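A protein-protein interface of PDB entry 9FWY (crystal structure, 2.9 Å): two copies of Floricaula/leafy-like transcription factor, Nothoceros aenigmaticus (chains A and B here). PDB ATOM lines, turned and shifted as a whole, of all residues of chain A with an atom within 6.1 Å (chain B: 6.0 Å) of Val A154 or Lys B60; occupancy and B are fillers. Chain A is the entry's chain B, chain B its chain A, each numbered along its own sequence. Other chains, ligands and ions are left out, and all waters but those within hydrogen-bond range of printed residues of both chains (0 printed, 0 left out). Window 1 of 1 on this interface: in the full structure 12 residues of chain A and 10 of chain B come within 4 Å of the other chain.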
ATOM      1  N   LYS A  64      -2.353  19.240 -18.632  1.00  0.00           N
ATOM      2  CA  LYS A  64      -2.841  18.670 -19.878  1.00  0.00           C
ATOM      3  C   LYS A  64      -4.204  18.028 -19.643  1.00  0.00           C
ATOM      4  O   LYS A  64      -4.599  17.803 -18.502  1.00  0.00           O
ATOM      5  CB  LYS A  64      -1.868  17.603 -20.403  1.00  0.00           C
ATOM      6  CG  LYS A  64      -0.445  18.093 -20.667  1.00  0.00           C
ATOM      7  CD  LYS A  64      -0.137  18.417 -22.120  1.00  0.00           C
ATOM      8  CE  LYS A  64       1.180  19.173 -22.181  1.00  0.00           C
ATOM      9  NZ  LYS A  64       1.697  19.312 -23.561  1.00  0.00           N
ATOM     10  N   VAL A  90      -7.021  15.430 -33.100  1.00  0.00           N
ATOM     11  CA  VAL A  90      -6.188  16.462 -32.499  1.00  0.00           C
ATOM     12  C   VAL A  90      -5.475  17.259 -33.586  1.00  0.00           C
ATOM     13  O   VAL A  90      -5.425  18.483 -33.519  1.00  0.00           O
ATOM     14  CB  VAL A  90      -5.121  15.947 -31.501  1.00  0.00           C
ATOM     15  CG1 VAL A  90      -4.582  17.091 -30.640  1.00  0.00           C
ATOM     16  CG2 VAL A  90      -5.652  14.838 -30.616  1.00  0.00           C
ATOM     17  N   ILE A 139       7.335  20.316 -34.357  1.00  0.00           N
ATOM     18  CA  ILE A 139       5.898  20.183 -34.162  1.00  0.00           C
ATOM     19  C   ILE A 139       5.500  20.251 -32.688  1.00  0.00           C
ATOM     20  O   ILE A 139       4.479  20.847 -32.343  1.00  0.00           O
ATOM     21  CB  ILE A 139       5.380  18.882 -34.835  1.00  0.00           C
ATOM     22  CG1 ILE A 139       3.837  18.828 -34.850  1.00  0.00           C
ATOM     23  CG2 ILE A 139       5.960  17.622 -34.188  1.00  0.00           C
ATOM     24  CD1 ILE A 139       3.168  19.975 -35.581  1.00  0.00           C
ATOM     25  N   GLU A 140       6.323  19.637 -31.828  1.00  0.00           N
ATOM     26  CA  GLU A 140       6.106  19.655 -30.391  1.00  0.00           C
ATOM     27  C   GLU A 140       6.203  21.093 -29.886  1.00  0.00           C
ATOM     28  O   GLU A 140       5.438  21.507 -29.012  1.00  0.00           O
ATOM     29  CB  GLU A 140       7.133  18.758 -29.689  1.00  0.00           C
ATOM     30  CG  GLU A 140       7.089  17.303 -30.126  1.00  0.00           C
ATOM     31  CD  GLU A 140       8.273  16.475 -29.666  1.00  0.00           C
ATOM     32  OE1 GLU A 140       9.410  16.766 -30.102  1.00  0.00           O
ATOM     33  OE2 GLU A 140       8.064  15.531 -28.869  1.00  0.00           O
ATOM     34  N   PHE A 143       2.892  23.023 -30.728  1.00  0.00           N
ATOM     35  CA  PHE A 143       1.910  22.721 -29.696  1.00  0.00           C
ATOM     36  C   PHE A 143       2.153  23.528 -28.420  1.00  0.00           C
ATOM     37  O   PHE A 143       1.225  24.126 -27.880  1.00  0.00           O
ATOM     38  CB  PHE A 143       1.889  21.212 -29.372  1.00  0.00           C
ATOM     39  CG  PHE A 143       0.940  20.404 -30.227  1.00  0.00           C
ATOM     40  CD1 PHE A 143       1.090  20.356 -31.602  1.00  0.00           C
ATOM     41  CD2 PHE A 143      -0.106  19.700 -29.654  1.00  0.00           C
ATOM     42  CE1 PHE A 143       0.211  19.615 -32.386  1.00  0.00           C
ATOM     43  CE2 PHE A 143      -0.981  18.962 -30.441  1.00  0.00           C
ATOM     44  CZ  PHE A 143      -0.820  18.926 -31.802  1.00  0.00           C
ATOM     45  N   ASN A 144       3.410  23.545 -27.956  1.00  0.00           N
ATOM     46  CA  ASN A 144       3.771  24.262 -26.740  1.00  0.00           C
ATOM     47  C   ASN A 144       3.764  25.784 -26.877  1.00  0.00           C
ATOM     48  O   ASN A 144       3.847  26.486 -25.871  1.00  0.00           O
ATOM     49  CB  ASN A 144       5.151  23.805 -26.243  1.00  0.00           C
ATOM     50  CG  ASN A 144       5.154  22.429 -25.620  1.00  0.00           C
ATOM     51  OD1 ASN A 144       4.108  21.802 -25.419  1.00  0.00           O
ATOM     52  ND2 ASN A 144       6.336  21.929 -25.285  1.00  0.00           N
ATOM     53  N   TRP A 152      -2.796  19.675 -24.903  1.00  0.00           N
ATOM     54  CA  TRP A 152      -3.024  18.423 -25.602  1.00  0.00           C
ATOM     55  C   TRP A 152      -1.705  17.702 -25.842  1.00  0.00           C
ATOM     56  O   TRP A 152      -0.743  18.308 -26.312  1.00  0.00           O
ATOM     57  CB  TRP A 152      -3.735  18.681 -26.925  1.00  0.00           C
ATOM     58  CG  TRP A 152      -5.061  19.340 -26.742  1.00  0.00           C
ATOM     59  CD1 TRP A 152      -5.368  20.644 -26.980  1.00  0.00           C
ATOM     60  CD2 TRP A 152      -6.260  18.722 -26.273  1.00  0.00           C
ATOM     61  NE1 TRP A 152      -6.688  20.878 -26.691  1.00  0.00           N
ATOM     62  CE2 TRP A 152      -7.262  19.713 -26.253  1.00  0.00           C
ATOM     63  CE3 TRP A 152      -6.589  17.423 -25.871  1.00  0.00           C
ATOM     64  CZ2 TRP A 152      -8.568  19.443 -25.842  1.00  0.00           C
ATOM     65  CZ3 TRP A 152      -7.881  17.157 -25.465  1.00  0.00           C
ATOM     66  CH2 TRP A 152      -8.854  18.159 -25.453  1.00  0.00           C
ATOM     67  N   TYR A 153      -1.675  16.406 -25.510  1.00  0.00           N
ATOM     68  CA  TYR A 153      -0.544  15.566 -25.852  1.00  0.00           C
ATOM     69  C   TYR A 153      -0.409  15.503 -27.370  1.00  0.00           C
ATOM     70  O   TYR A 153      -1.408  15.410 -28.081  1.00  0.00           O
ATOM     71  CB  TYR A 153      -0.694  14.155 -25.294  1.00  0.00           C
ATOM     72  CG  TYR A 153      -0.629  14.058 -23.789  1.00  0.00           C
ATOM     73  CD1 TYR A 153       0.346  14.736 -23.067  1.00  0.00           C
ATOM     74  CD2 TYR A 153      -1.514  13.254 -23.088  1.00  0.00           C
ATOM     75  CE1 TYR A 153       0.426  14.627 -21.685  1.00  0.00           C
ATOM     76  CE2 TYR A 153      -1.448  13.141 -21.705  1.00  0.00           C
ATOM     77  CZ  TYR A 153      -0.477  13.828 -21.006  1.00  0.00           C
ATOM     78  OH  TYR A 153      -0.419  13.715 -19.637  1.00  0.00           O
ATOM     79  N   VAL A 154       0.839  15.561 -27.843  1.00  0.00           N
ATOM     80  CA  VAL A 154       1.115  15.553 -29.268  1.00  0.00           C
ATOM     81  C   VAL A 154       1.146  14.080 -29.661  1.00  0.00           C
ATOM     82  O   VAL A 154       1.879  13.307 -29.048  1.00  0.00           O
ATOM     83  CB  VAL A 154       2.421  16.283 -29.655  1.00  0.00           C
ATOM     84  CG1 VAL A 154       2.322  16.815 -31.077  1.00  0.00           C
ATOM     85  CG2 VAL A 154       2.769  17.415 -28.684  1.00  0.00           C
ATOM     86  N   PRO A 155       0.325  13.630 -30.639  1.00  0.00           N
ATOM     87  CA  PRO A 155       0.330  12.225 -31.055  1.00  0.00           C
ATOM     88  C   PRO A 155       1.660  11.775 -31.650  1.00  0.00           C
ATOM     89  O   PRO A 155       2.298  12.533 -32.380  1.00  0.00           O
ATOM     90  CB  PRO A 155      -0.792  12.163 -32.100  1.00  0.00           C
ATOM     91  CG  PRO A 155      -1.635  13.387 -31.851  1.00  0.00           C
ATOM     92  CD  PRO A 155      -0.689  14.426 -31.350  1.00  0.00           C
ATOM     93  N   LYS A 156       2.067  10.540 -31.321  1.00  0.00           N
ATOM     94  CA  LYS A 156       3.233   9.914 -31.929  1.00  0.00           C
ATOM     95  C   LYS A 156       3.228  10.098 -33.443  1.00  0.00           C
ATOM     96  O   LYS A 156       4.220  10.539 -34.018  1.00  0.00           O
ATOM     97  CB  LYS A 156       3.280   8.396 -31.659  1.00  0.00           C
ATOM     98  CG  LYS A 156       3.728   7.979 -30.278  1.00  0.00           C
ATOM     99  CD  LYS A 156       3.727   6.451 -30.148  1.00  0.00           C
ATOM    100  CE  LYS A 156       3.908   5.964 -28.731  1.00  0.00           C
ATOM    101  NZ  LYS A 156       3.576   4.516 -28.606  1.00  0.00           N
ATOM    102  N   LEU A 158       1.907  12.117 -35.607  1.00  0.00           N
ATOM    103  CA  LEU A 158       2.219  13.424 -36.162  1.00  0.00           C
ATOM    104  C   LEU A 158       3.723  13.693 -36.123  1.00  0.00           C
ATOM    105  O   LEU A 158       4.298  14.163 -37.107  1.00  0.00           O
ATOM    106  CB  LEU A 158       1.452  14.516 -35.406  1.00  0.00           C
ATOM    107  CG  LEU A 158       1.658  15.942 -35.905  1.00  0.00           C
ATOM    108  CD1 LEU A 158       1.132  16.104 -37.313  1.00  0.00           C
ATOM    109  CD2 LEU A 158       1.003  16.937 -34.977  1.00  0.00           C
ATOM    110  N   ILE A 159       4.355  13.373 -34.984  1.00  0.00           N
ATOM    111  CA  ILE A 159       5.791  13.554 -34.831  1.00  0.00           C
ATOM    112  C   ILE A 159       6.518  12.728 -35.888  1.00  0.00           C
ATOM    113  O   ILE A 159       7.376  13.245 -36.600  1.00  0.00           O
ATOM    114  CB  ILE A 159       6.292  13.182 -33.414  1.00  0.00           C
ATOM    115  CG1 ILE A 159       5.510  13.903 -32.306  1.00  0.00           C
ATOM    116  CG2 ILE A 159       7.792  13.460 -33.281  1.00  0.00           C
ATOM    117  CD1 ILE A 159       5.811  13.395 -30.950  1.00  0.00           C
ATOM    118  N   ALA B  54      15.995  11.316 -29.243  1.00  0.00           N
ATOM    119  CA  ALA B  54      14.598  11.222 -29.633  1.00  0.00           C
ATOM    120  C   ALA B  54      14.290  12.074 -30.865  1.00  0.00           C
ATOM    121  O   ALA B  54      13.608  11.616 -31.778  1.00  0.00           O
ATOM    122  CB  ALA B  54      13.704  11.639 -28.472  1.00  0.00           C
ATOM    123  N   GLY B  58      13.016  10.857 -34.382  1.00  0.00           N
ATOM    124  CA  GLY B  58      11.649  11.278 -34.649  1.00  0.00           C
ATOM    125  C   GLY B  58      10.638  10.655 -33.689  1.00  0.00           C
ATOM    126  O   GLY B  58       9.517  10.350 -34.085  1.00  0.00           O
ATOM    127  N   GLU B  59      11.058  10.474 -32.430  1.00  0.00           N
ATOM    128  CA  GLU B  59      10.211   9.942 -31.376  1.00  0.00           C
ATOM    129  C   GLU B  59       9.733  11.075 -30.470  1.00  0.00           C
ATOM    130  O   GLU B  59      10.166  12.217 -30.620  1.00  0.00           O
ATOM    131  CB  GLU B  59      10.984   8.902 -30.555  1.00  0.00           C
ATOM    132  CG  GLU B  59      11.444   7.710 -31.373  1.00  0.00           C
ATOM    133  CD  GLU B  59      12.280   6.693 -30.621  1.00  0.00           C
ATOM    134  OE1 GLU B  59      12.900   7.050 -29.592  1.00  0.00           O
ATOM    135  OE2 GLU B  59      12.298   5.523 -31.062  1.00  0.00           O
ATOM    136  N   LYS B  60       8.839  10.746 -29.530  1.00  0.00           N
ATOM    137  CA  LYS B  60       8.335  11.730 -28.583  1.00  0.00           C
ATOM    138  C   LYS B  60       9.478  12.167 -27.667  1.00  0.00           C
ATOM    139  O   LYS B  60      10.305  11.348 -27.267  1.00  0.00           O
ATOM    140  CB  LYS B  60       7.154  11.172 -27.775  1.00  0.00           C
ATOM    141  CG  LYS B  60       6.142  12.242 -27.368  1.00  0.00           C
ATOM    142  CD  LYS B  60       4.957  11.689 -26.579  1.00  0.00           C
ATOM    143  CE  LYS B  60       3.962  12.768 -26.191  1.00  0.00           C
ATOM    144  NZ  LYS B  60       2.890  12.248 -25.294  1.00  0.00           N
ATOM    145  N   CYS B  61       9.511  13.468 -27.353  1.00  0.00           N
ATOM    146  CA  CYS B  61      10.631  14.090 -26.662  1.00  0.00           C
ATOM    147  C   CYS B  61      10.232  14.508 -25.247  1.00  0.00           C
ATOM    148  O   CYS B  61       9.409  15.407 -25.083  1.00  0.00           O
ATOM    149  CB  CYS B  61      11.136  15.280 -27.471  1.00  0.00           C
ATOM    150  SG  CYS B  61      12.557  16.130 -26.739  1.00  0.00           S
ATOM    151  N   PRO B  62      10.810  13.895 -24.183  1.00  0.00           N
ATOM    152  CA  PRO B  62      10.384  14.166 -22.809  1.00  0.00           C
ATOM    153  C   PRO B  62      10.876  15.503 -22.264  1.00  0.00           C
ATOM    154  O   PRO B  62      11.996  15.920 -22.551  1.00  0.00           O
ATOM    155  CB  PRO B  62      10.993  12.998 -22.030  1.00  0.00           C
ATOM    156  CG  PRO B  62      12.236  12.663 -22.793  1.00  0.00           C
ATOM    157  CD  PRO B  62      11.906  12.913 -24.245  1.00  0.00           C
ATOM    158  N   GLN B  68      12.493   6.569 -18.700  1.00  0.00           N
ATOM    159  CA  GLN B  68      13.335   6.473 -19.880  1.00  0.00           C
ATOM    160  C   GLN B  68      14.718   7.069 -19.622  1.00  0.00           C
ATOM    161  O   GLN B  68      15.728   6.445 -19.946  1.00  0.00           O
ATOM    162  CB  GLN B  68      12.663   7.183 -21.065  1.00  0.00           C
ATOM    163  CG  GLN B  68      13.345   6.944 -22.402  1.00  0.00           C
ATOM    164  CD  GLN B  68      12.798   7.832 -23.489  1.00  0.00           C
ATOM    165  OE1 GLN B  68      11.858   8.605 -23.288  1.00  0.00           O
ATOM    166  NE2 GLN B  68      13.378   7.738 -24.673  1.00  0.00           N
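The side-chain carboxylate (OE2) of Glu A140 lies within hydrogen-bond range of the backbone NH (N) of Cys B61, at 2.9 Å.
The backbone carbonyl oxygen (O) of Ala B54 lies within hydrogen-bond range of the backbone NH (N) of Glu B59.
Among the printed residues, pairs that only touch across the chains: Val A154 with Lys B60, Ile A159 with Gly B58, Ile A159 with Glu B59, Ile A159 with Lys B60 and Glu A140 with Lys B60.
Val A154 touches just one residue of chain B: Lys B60 (3.6 Å). Of the printed residues of chain A, Glu B59 touches Ile A159 (3.8 Å). Of the printed residues of chain B, Ile A159 touches Gly B58, Glu B59 and Lys B60. Of the printed residues of chain A, Cys B61 touches Glu A140 (2.9 Å). Lys A64 touches none of the printed residues of chain B. The nearest printed residue of chain B that does not touch Val A154 is Cys B61 (7.8 Å).
Printed residues of chain A that touch a printed residue of chain B: Glu A140, Val A154 and Ile A159. Printed residues of chain B that touch a printed residue of chain A: Gly B58, Glu B59, Lys B60 and Cys B61. Among the printed residues, 6 pairs touch across the chains.
No position is printed for both chains.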
